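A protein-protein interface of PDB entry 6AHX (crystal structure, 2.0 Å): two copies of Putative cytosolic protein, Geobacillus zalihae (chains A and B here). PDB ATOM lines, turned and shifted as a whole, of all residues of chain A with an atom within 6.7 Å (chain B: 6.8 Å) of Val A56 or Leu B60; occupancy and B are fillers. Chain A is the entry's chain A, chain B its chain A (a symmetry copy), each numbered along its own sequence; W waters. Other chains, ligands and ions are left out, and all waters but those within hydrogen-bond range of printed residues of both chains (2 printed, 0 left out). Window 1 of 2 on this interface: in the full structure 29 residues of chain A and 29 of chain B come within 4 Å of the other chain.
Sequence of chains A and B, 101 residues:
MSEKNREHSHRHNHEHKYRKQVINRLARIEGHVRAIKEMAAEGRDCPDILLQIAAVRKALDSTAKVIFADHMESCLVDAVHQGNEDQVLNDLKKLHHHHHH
The backbone carbonyl oxygen (O) of Arg B57 lies within hydrogen-bond range of the guanidinium group (NE) of Arg A57 (2.9 Å).
The side-chain carboxylate of Asp B61 lies within salt-bridge range of the side-chain amino group of Lys B65.
O of Leu B26 touches CG1 of Val A33, 3.6 Å away.
O of Ile A36 touches CD1 of Leu B26, 3.9 Å away.
CG2 of Ile A53 touches O of Leu B60, at 3.6 Å.
CD1 of Leu B60 touches CG1 of Val A56, at 3.4 Å.
Leu B60 touches Arg A57.
Arg A57 touches Asp B61.
CD1 of Leu A60 touches CG1 of Val B56, 3.4 Å away.
Leu A60 touches Arg B57 (CB to CG, 3.8 Å).
Leu A60 touches Leu B60.
Arg B57 touches Asp A61.
Printed residues of chain B within 4 Å of Val A56: Leu B60.
Of the printed residues of chain B, Val A33 touches Leu B26.
Of the printed residues of chain A, Asp B61 touches Arg A57.
Of the printed residues of chain B, Ile A36 touches Leu B26.
Ile B29 touches none of the printed residues of chain A.
Lys B65 touches none of the printed residues of chain A.
Of the 15 printed residues of chain A, 7 touch a printed residue of chain B.
Hydrophobic or aromatic side chains of chain B within 4 Å of the printed part of chain A: Leu B26, Val B56 and Leu B60.
Among the printed residues, 11 pairs touch across the chains.
Val A56 touches Leu B60, and with the chains exchanged Leu A60 touches Val B56.
Arg B57 touches its own counterpart, Arg A57.
Arg A57 touches Asp B61, and with the chains exchanged Asp A61 touches Arg B57.
Leu A60 touches its own counterpart, Leu B60.
Positions printed for both chains: 29, 33, 55, 56, 57, 58, 59, 60 and 61.
Of the 11 pairs that touch across the chains among the printed residues, 8 have their exchanged pair printed and touching as well.
Water W1 bridges NH2 of Arg B57 (2.9 Å) and N of Lys A58 (3.4 Å).
Water W2 lies within hydrogen-bond range of the guanidinium group (NH2) of Arg A57 (2.9 Å) and the backbone NH (N) of Lys B58 (3.4 Å).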
ATOM      1  N   ILE A  29     -15.585   7.994  21.211  1.00  0.00           N
ATOM      2  CA  ILE A  29     -16.552   7.669  22.228  1.00  0.00           C
ATOM      3  C   ILE A  29     -16.078   8.263  23.530  1.00  0.00           C
ATOM      4  O   ILE A  29     -16.860   8.820  24.280  1.00  0.00           O
ATOM      5  CB  ILE A  29     -16.769   6.156  22.373  1.00  0.00           C
ATOM      6  CG1 ILE A  29     -17.419   5.564  21.141  1.00  0.00           C
ATOM      7  CG2 ILE A  29     -17.699   5.891  23.562  1.00  0.00           C
ATOM      8  CD1 ILE A  29     -17.224   4.107  21.035  1.00  0.00           C
ATOM      9  N   HIS A  32     -16.845  11.926  23.527  1.00  0.00           N
ATOM     10  CA  HIS A  32     -18.307  12.045  23.507  1.00  0.00           C
ATOM     11  C   HIS A  32     -18.807  11.950  24.951  1.00  0.00           C
ATOM     12  O   HIS A  32     -19.565  12.796  25.410  1.00  0.00           O
ATOM     13  CB  HIS A  32     -18.840  10.989  22.545  1.00  0.00           C
ATOM     14  CG  HIS A  32     -20.259  11.178  22.122  1.00  0.00           C
ATOM     15  ND1 HIS A  32     -21.119  12.095  22.697  1.00  0.00           N
ATOM     16  CD2 HIS A  32     -20.986  10.496  21.241  1.00  0.00           C
ATOM     17  CE1 HIS A  32     -22.315  11.959  22.182  1.00  0.00           C
ATOM     18  NE2 HIS A  32     -22.252  11.006  21.281  1.00  0.00           N
ATOM     19  N   VAL A  33     -18.340  10.979  25.687  1.00  0.00           N
ATOM     20  CA  VAL A  33     -18.716  10.867  27.124  1.00  0.00           C
ATOM     21  C   VAL A  33     -18.265  12.091  27.931  1.00  0.00           C
ATOM     22  O   VAL A  33     -19.055  12.609  28.788  1.00  0.00           O
ATOM     23  CB  VAL A  33     -18.245   9.539  27.819  1.00  0.00           C
ATOM     24  CG1 VAL A  33     -18.774   9.503  29.254  1.00  0.00           C
ATOM     25  CG2 VAL A  33     -18.746   8.288  27.125  1.00  0.00           C
ATOM     26  N   ILE A  36     -20.772  14.726  27.303  1.00  0.00           N
ATOM     27  CA  ILE A  36     -21.987  14.394  28.043  1.00  0.00           C
ATOM     28  C   ILE A  36     -21.836  14.746  29.509  1.00  0.00           C
ATOM     29  O   ILE A  36     -22.741  15.315  30.113  1.00  0.00           O
ATOM     30  CB  ILE A  36     -22.426  12.909  27.882  1.00  0.00           C
ATOM     31  CG1 ILE A  36     -22.711  12.539  26.398  1.00  0.00           C
ATOM     32  CG2 ILE A  36     -23.673  12.641  28.745  1.00  0.00           C
ATOM     33  CD1 ILE A  36     -23.016  11.078  26.172  1.00  0.00           C
ATOM     34  N   LEU A  51     -30.485  11.551  25.042  1.00  0.00           N
ATOM     35  CA  LEU A  51     -30.188  11.304  23.638  1.00  0.00           C
ATOM     36  C   LEU A  51     -28.752  10.922  23.371  1.00  0.00           C
ATOM     37  O   LEU A  51     -28.486  10.006  22.624  1.00  0.00           O
ATOM     38  CB  LEU A  51     -30.508  12.559  22.789  1.00  0.00           C
ATOM     39  CG  LEU A  51     -30.682  12.322  21.301  1.00  0.00           C
ATOM     40  CD1 LEU A  51     -32.100  11.790  21.067  1.00  0.00           C
ATOM     41  CD2 LEU A  51     -30.397  13.579  20.484  1.00  0.00           C
ATOM     42  N   GLN A  52     -27.832  11.624  24.022  1.00  0.00           N
ATOM     43  CA  GLN A  52     -26.409  11.406  23.795  1.00  0.00           C
ATOM     44  C   GLN A  52     -25.953  10.161  24.487  1.00  0.00           C
ATOM     45  O   GLN A  52     -25.162   9.425  23.894  1.00  0.00           O
ATOM     46  CB  GLN A  52     -25.588  12.625  24.212  1.00  0.00           C
ATOM     47  CG  GLN A  52     -25.924  13.874  23.411  1.00  0.00           C
ATOM     48  CD  GLN A  52     -25.835  13.710  21.901  1.00  0.00           C
ATOM     49  OE1 GLN A  52     -25.149  12.835  21.373  1.00  0.00           O
ATOM     50  NE2 GLN A  52     -26.617  14.497  21.205  1.00  0.00           N
ATOM     51  N   ILE A  53     -26.542   9.830  25.639  1.00  0.00           N
ATOM     52  CA  ILE A  53     -26.193   8.575  26.256  1.00  0.00           C
ATOM     53  C   ILE A  53     -26.560   7.402  25.361  1.00  0.00           C
ATOM     54  O   ILE A  53     -25.827   6.394  25.258  1.00  0.00           O
ATOM     55  CB  ILE A  53     -26.813   8.420  27.647  1.00  0.00           C
ATOM     56  CG1 ILE A  53     -26.151   9.425  28.626  1.00  0.00           C
ATOM     57  CG2 ILE A  53     -26.563   7.017  28.216  1.00  0.00           C
ATOM     58  CD1 ILE A  53     -26.746   9.501  30.026  1.00  0.00           C
ATOM     59  N   ALA A  54     -27.754   7.471  24.806  1.00  0.00           N
ATOM     60  CA  ALA A  54     -28.192   6.415  23.930  1.00  0.00           C
ATOM     61  C   ALA A  54     -27.292   6.327  22.701  1.00  0.00           C
ATOM     62  O   ALA A  54     -26.962   5.231  22.256  1.00  0.00           O
ATOM     63  CB  ALA A  54     -29.595   6.628  23.526  1.00  0.00           C
ATOM     64  N   ALA A  55     -26.911   7.453  22.139  1.00  0.00           N
ATOM     65  CA  ALA A  55     -25.958   7.438  21.024  1.00  0.00           C
ATOM     66  C   ALA A  55     -24.619   6.770  21.384  1.00  0.00           C
ATOM     67  O   ALA A  55     -24.126   5.953  20.654  1.00  0.00           O
ATOM     68  CB  ALA A  55     -25.740   8.836  20.554  1.00  0.00           C
ATOM     69  N   VAL A  56     -24.079   7.056  22.554  1.00  0.00           N
ATOM     70  CA  VAL A  56     -22.876   6.395  23.002  1.00  0.00           C
ATOM     71  C   VAL A  56     -23.045   4.878  23.185  1.00  0.00           C
ATOM     72  O   VAL A  56     -22.165   4.111  22.809  1.00  0.00           O
ATOM     73  CB  VAL A  56     -22.341   7.045  24.308  1.00  0.00           C
ATOM     74  CG1 VAL A  56     -21.167   6.241  24.861  1.00  0.00           C
ATOM     75  CG2 VAL A  56     -21.885   8.484  24.068  1.00  0.00           C
ATOM     76  N   ARG A  57     -24.157   4.429  23.788  1.00  0.00           N
ATOM     77  CA  ARG A  57     -24.457   2.978  23.896  1.00  0.00           C
ATOM     78  C   ARG A  57     -24.481   2.274  22.533  1.00  0.00           C
ATOM     79  O   ARG A  57     -24.003   1.159  22.371  1.00  0.00           O
ATOM     80  CB  ARG A  57     -25.727   2.737  24.713  1.00  0.00           C
ATOM     81  CG  ARG A  57     -25.578   3.194  26.194  1.00  0.00           C
ATOM     82  CD  ARG A  57     -26.756   2.756  27.098  1.00  0.00           C
ATOM     83  NE  ARG A  57     -26.790   1.287  27.326  1.00  0.00           N
ATOM     84  CZ  ARG A  57     -27.633   0.428  26.758  1.00  0.00           C
ATOM     85  NH1 ARG A  57     -28.528   0.830  25.924  1.00  0.00           N
ATOM     86  NH2 ARG A  57     -27.574  -0.874  27.027  1.00  0.00           N
ATOM     87  N   LYS A  58     -25.036   2.962  21.550  1.00  0.00           N
ATOM     88  CA  LYS A  58     -25.071   2.450  20.194  1.00  0.00           C
ATOM     89  C   LYS A  58     -23.685   2.395  19.543  1.00  0.00           C
ATOM     90  O   LYS A  58     -23.370   1.383  18.942  1.00  0.00           O
ATOM     91  CB  LYS A  58     -26.044   3.296  19.412  1.00  0.00           C
ATOM     92  CG  LYS A  58     -26.290   2.802  18.026  1.00  0.00           C
ATOM     93  CD  LYS A  58     -27.304   3.710  17.327  1.00  0.00           C
ATOM     94  CE  LYS A  58     -27.890   3.028  16.075  1.00  0.00           C
ATOM     95  NZ  LYS A  58     -27.759   3.934  14.890  1.00  0.00           N
ATOM     96  N   ALA A  59     -22.852   3.424  19.726  1.00  0.00           N
ATOM     97  CA  ALA A  59     -21.503   3.475  19.205  1.00  0.00           C
ATOM     98  C   ALA A  59     -20.655   2.385  19.806  1.00  0.00           C
ATOM     99  O   ALA A  59     -19.852   1.731  19.101  1.00  0.00           O
ATOM    100  CB  ALA A  59     -20.879   4.828  19.504  1.00  0.00           C
ATOM    101  N   LEU A  60     -20.839   2.169  21.105  1.00  0.00           N
ATOM    102  CA  LEU A  60     -20.120   1.102  21.813  1.00  0.00           C
ATOM    103  C   LEU A  60     -20.532  -0.312  21.316  1.00  0.00           C
ATOM    104  O   LEU A  60     -19.706  -1.188  21.108  1.00  0.00           O
ATOM    105  CB  LEU A  60     -20.309   1.214  23.344  1.00  0.00           C
ATOM    106  CG  LEU A  60     -19.469   2.281  24.099  1.00  0.00           C
ATOM    107  CD1 LEU A  60     -20.071   2.595  25.459  1.00  0.00           C
ATOM    108  CD2 LEU A  60     -17.986   1.925  24.304  1.00  0.00           C
ATOM    109  N   ASP A  61     -21.809  -0.519  21.162  1.00  0.00           N
ATOM    110  CA  ASP A  61     -22.346  -1.710  20.551  1.00  0.00           C
ATOM    111  C   ASP A  61     -21.764  -1.938  19.151  1.00  0.00           C
ATOM    112  O   ASP A  61     -21.293  -3.003  18.875  1.00  0.00           O
ATOM    113  CB  ASP A  61     -23.860  -1.641  20.531  1.00  0.00           C
ATOM    114  CG  ASP A  61     -24.488  -2.900  19.929  1.00  0.00           C
ATOM    115  OD1 ASP A  61     -24.404  -3.951  20.524  1.00  0.00           O
ATOM    116  OD2 ASP A  61     -25.016  -2.863  18.812  1.00  0.00           O
ATOM    117  N   ARG B  25     -20.318   9.883  37.991  1.00  0.00           N
ATOM    118  CA  ARG B  25     -20.477   8.637  37.237  1.00  0.00           C
ATOM    119  C   ARG B  25     -20.050   8.847  35.772  1.00  0.00           C
ATOM    120  O   ARG B  25     -19.264   8.059  35.226  1.00  0.00           O
ATOM    121  CB  ARG B  25     -21.891   8.091  37.330  1.00  0.00           C
ATOM    122  CG  ARG B  25     -21.893   6.615  37.745  1.00  0.00           C
ATOM    123  CD  ARG B  25     -21.315   5.482  36.815  1.00  0.00           C
ATOM    124  NE  ARG B  25     -22.378   4.434  36.910  1.00  0.00           N
ATOM    125  CZ  ARG B  25     -22.282   3.105  37.141  1.00  0.00           C
ATOM    126  NH1 ARG B  25     -21.144   2.430  37.163  1.00  0.00           N
ATOM    127  NH2 ARG B  25     -23.408   2.399  37.272  1.00  0.00           N
ATOM    128  N   LEU B  26     -20.507   9.954  35.186  1.00  0.00           N
ATOM    129  CA  LEU B  26     -20.154  10.257  33.835  1.00  0.00           C
ATOM    130  C   LEU B  26     -18.661  10.437  33.705  1.00  0.00           C
ATOM    131  O   LEU B  26     -18.072   9.983  32.718  1.00  0.00           O
ATOM    132  CB  LEU B  26     -20.930  11.482  33.301  1.00  0.00           C
ATOM    133  CG  LEU B  26     -22.396  11.192  32.946  1.00  0.00           C
ATOM    134  CD1 LEU B  26     -23.149  12.513  32.745  1.00  0.00           C
ATOM    135  CD2 LEU B  26     -22.612  10.256  31.741  1.00  0.00           C
ATOM    136  N   ILE B  29     -17.127   6.834  33.815  1.00  0.00           N
ATOM    137  CA  ILE B  29     -17.381   6.178  32.559  1.00  0.00           C
ATOM    138  C   ILE B  29     -16.422   6.736  31.537  1.00  0.00           C
ATOM    139  O   ILE B  29     -15.862   6.001  30.744  1.00  0.00           O
ATOM    140  CB  ILE B  29     -18.831   6.349  32.086  1.00  0.00           C
ATOM    141  CG1 ILE B  29     -19.805   5.635  32.999  1.00  0.00           C
ATOM    142  CG2 ILE B  29     -18.980   5.745  30.685  1.00  0.00           C
ATOM    143  CD1 ILE B  29     -21.183   6.139  32.874  1.00  0.00           C
ATOM    144  N   VAL B  33     -13.749   4.350  29.461  1.00  0.00           N
ATOM    145  CA  VAL B  33     -13.591   4.287  27.982  1.00  0.00           C
ATOM    146  C   VAL B  33     -12.151   4.584  27.546  1.00  0.00           C
ATOM    147  O   VAL B  33     -11.605   3.870  26.641  1.00  0.00           O
ATOM    148  CB  VAL B  33     -14.609   5.175  27.179  1.00  0.00           C
ATOM    149  CG1 VAL B  33     -14.408   4.947  25.680  1.00  0.00           C
ATOM    150  CG2 VAL B  33     -16.059   4.857  27.490  1.00  0.00           C
ATOM    151  N   ALA B  55     -19.539  -3.676  30.190  1.00  0.00           N
ATOM    152  CA  ALA B  55     -19.636  -2.972  31.472  1.00  0.00           C
ATOM    153  C   ALA B  55     -19.939  -1.472  31.316  1.00  0.00           C
ATOM    154  O   ALA B  55     -20.798  -0.949  31.975  1.00  0.00           O
ATOM    155  CB  ALA B  55     -18.370  -3.176  32.234  1.00  0.00           C
ATOM    156  N   VAL B  56     -19.293  -0.803  30.378  1.00  0.00           N
ATOM    157  CA  VAL B  56     -19.595   0.583  30.108  1.00  0.00           C
ATOM    158  C   VAL B  56     -21.033   0.808  29.610  1.00  0.00           C
ATOM    159  O   VAL B  56     -21.688   1.755  30.030  1.00  0.00           O
ATOM    160  CB  VAL B  56     -18.571   1.187  29.109  1.00  0.00           C
ATOM    161  CG1 VAL B  56     -18.990   2.598  28.704  1.00  0.00           C
ATOM    162  CG2 VAL B  56     -17.169   1.243  29.713  1.00  0.00           C
ATOM    163  N   ARG B  57     -21.528  -0.036  28.691  1.00  0.00           N
ATOM    164  CA  ARG B  57     -22.944   0.035  28.247  1.00  0.00           C
ATOM    165  C   ARG B  57     -23.937  -0.080  29.409  1.00  0.00           C
ATOM    166  O   ARG B  57     -24.950   0.605  29.466  1.00  0.00           O
ATOM    167  CB  ARG B  57     -23.220  -0.969  27.126  1.00  0.00           C
ATOM    168  CG  ARG B  57     -22.411  -0.654  25.833  1.00  0.00           C
ATOM    169  CD  ARG B  57     -22.838  -1.508  24.614  1.00  0.00           C
ATOM    170  NE  ARG B  57     -24.194  -1.157  24.112  1.00  0.00           N
ATOM    171  CZ  ARG B  57     -25.303  -1.868  24.298  1.00  0.00           C
ATOM    172  NH1 ARG B  57     -25.281  -2.972  24.961  1.00  0.00           N
ATOM    173  NH2 ARG B  57     -26.472  -1.458  23.811  1.00  0.00           N
ATOM    174  N   LYS B  58     -23.613  -0.954  30.347  1.00  0.00           N
ATOM    175  CA  LYS B  58     -24.425  -1.123  31.537  1.00  0.00           C
ATOM    176  C   LYS B  58     -24.369   0.091  32.471  1.00  0.00           C
ATOM    177  O   LYS B  58     -25.416   0.514  32.928  1.00  0.00           O
ATOM    178  CB  LYS B  58     -23.980  -2.394  32.216  1.00  0.00           C
ATOM    179  CG  LYS B  58     -24.820  -2.774  33.387  1.00  0.00           C
ATOM    180  CD  LYS B  58     -24.307  -4.084  33.989  1.00  0.00           C
ATOM    181  CE  LYS B  58     -25.358  -4.719  34.919  1.00  0.00           C
ATOM    182  NZ  LYS B  58     -24.745  -5.026  36.251  1.00  0.00           N
ATOM    183  N   ALA B  59     -23.190   0.681  32.683  1.00  0.00           N
ATOM    184  CA  ALA B  59     -23.012   1.859  33.504  1.00  0.00           C
ATOM    185  C   ALA B  59     -23.753   3.035  32.924  1.00  0.00           C
ATOM    186  O   ALA B  59     -24.392   3.821  33.661  1.00  0.00           O
ATOM    187  CB  ALA B  59     -21.533   2.198  33.617  1.00  0.00           C
ATOM    188  N   LEU B  60     -23.691   3.153  31.601  1.00  0.00           N
ATOM    189  CA  LEU B  60     -24.411   4.220  30.893  1.00  0.00           C
ATOM    190  C   LEU B  60     -25.953   4.062  31.006  1.00  0.00           C
ATOM    191  O   LEU B  60     -26.683   5.014  31.233  1.00  0.00           O
ATOM    192  CB  LEU B  60     -23.981   4.301  29.409  1.00  0.00           C
ATOM    193  CG  LEU B  60     -22.632   4.995  29.084  1.00  0.00           C
ATOM    194  CD1 LEU B  60     -22.128   4.602  27.704  1.00  0.00           C
ATOM    195  CD2 LEU B  60     -22.647   6.533  29.166  1.00  0.00           C
ATOM    196  N   ASP B  61     -26.425   2.861  30.817  1.00  0.00           N
ATOM    197  CA  ASP B  61     -27.804   2.511  31.051  1.00  0.00           C
ATOM    198  C   ASP B  61     -28.239   2.857  32.480  1.00  0.00           C
ATOM    199  O   ASP B  61     -29.232   3.502  32.654  1.00  0.00           O
ATOM    200  CB  ASP B  61     -28.025   1.047  30.730  1.00  0.00           C
ATOM    201  CG  ASP B  61     -29.483   0.627  30.924  1.00  0.00           C
ATOM    202  OD1 ASP B  61     -30.333   1.063  30.178  1.00  0.00           O
ATOM    203  OD2 ASP B  61     -29.807  -0.095  31.873  1.00  0.00           O
ATOM    204  N   SER B  62     -27.459   2.550  33.498  1.00  0.00           N
ATOM    205  CA  SER B  62     -27.842   2.929  34.858  1.00  0.00           C
ATOM    206  C   SER B  62     -27.869   4.397  35.131  1.00  0.00           C
ATOM    207  O   SER B  62     -28.738   4.902  35.831  1.00  0.00           O
ATOM    208  CB  SER B  62     -26.907   2.293  35.857  1.00  0.00           C
ATOM    209  OG  SER B  62     -27.146   0.922  35.701  1.00  0.00           O
ATOM    210  N   THR B  63     -26.874   5.068  34.615  1.00  0.00           N
ATOM    211  CA  THR B  63     -26.826   6.487  34.676  1.00  0.00           C
ATOM    212  C   THR B  63     -28.027   7.175  34.007  1.00  0.00           C
ATOM    213  O   THR B  63     -28.518   8.102  34.561  1.00  0.00           O
ATOM    214  CB  THR B  63     -25.482   6.993  34.088  1.00  0.00           C
ATOM    215  OG1 THR B  63     -24.443   6.351  34.805  1.00  0.00           O
ATOM    216  CG2 THR B  63     -25.362   8.478  34.240  1.00  0.00           C
ATOM    217  N   ALA B  64     -28.448   6.756  32.825  1.00  0.00           N
ATOM    218  CA  ALA B  64     -29.660   7.278  32.195  1.00  0.00           C
ATOM    219  C   ALA B  64     -30.957   7.087  33.046  1.00  0.00           C
ATOM    220  O   ALA B  64     -31.805   8.001  33.171  1.00  0.00           O
ATOM    221  CB  ALA B  64     -29.862   6.589  30.846  1.00  0.00           C
ATOM    222  N   LYS B  65     -31.065   5.890  33.632  1.00  0.00           N
ATOM    223  CA  LYS B  65     -32.125   5.573  34.595  1.00  0.00           C
ATOM    224  C   LYS B  65     -32.124   6.494  35.820  1.00  0.00           C
ATOM    225  O   LYS B  65     -33.141   6.989  36.192  1.00  0.00           O
ATOM    226  CB  LYS B  65     -32.013   4.151  35.034  1.00  0.00           C
ATOM    227  CG  LYS B  65     -32.364   3.168  33.943  1.00  0.00           C
ATOM    228  CD  LYS B  65     -32.198   1.775  34.553  1.00  0.00           C
ATOM    229  CE  LYS B  65     -32.304   0.595  33.585  1.00  0.00           C
ATOM    230  NZ  LYS B  65     -32.980   0.890  32.292  1.00  0.00           N
HETATM  231  O   HOH W   1     -27.458   0.653  22.006  1.00  0.00           O
HETATM  232  O   HOH W   2     -26.162  -2.644  28.916  1.00  0.00           O
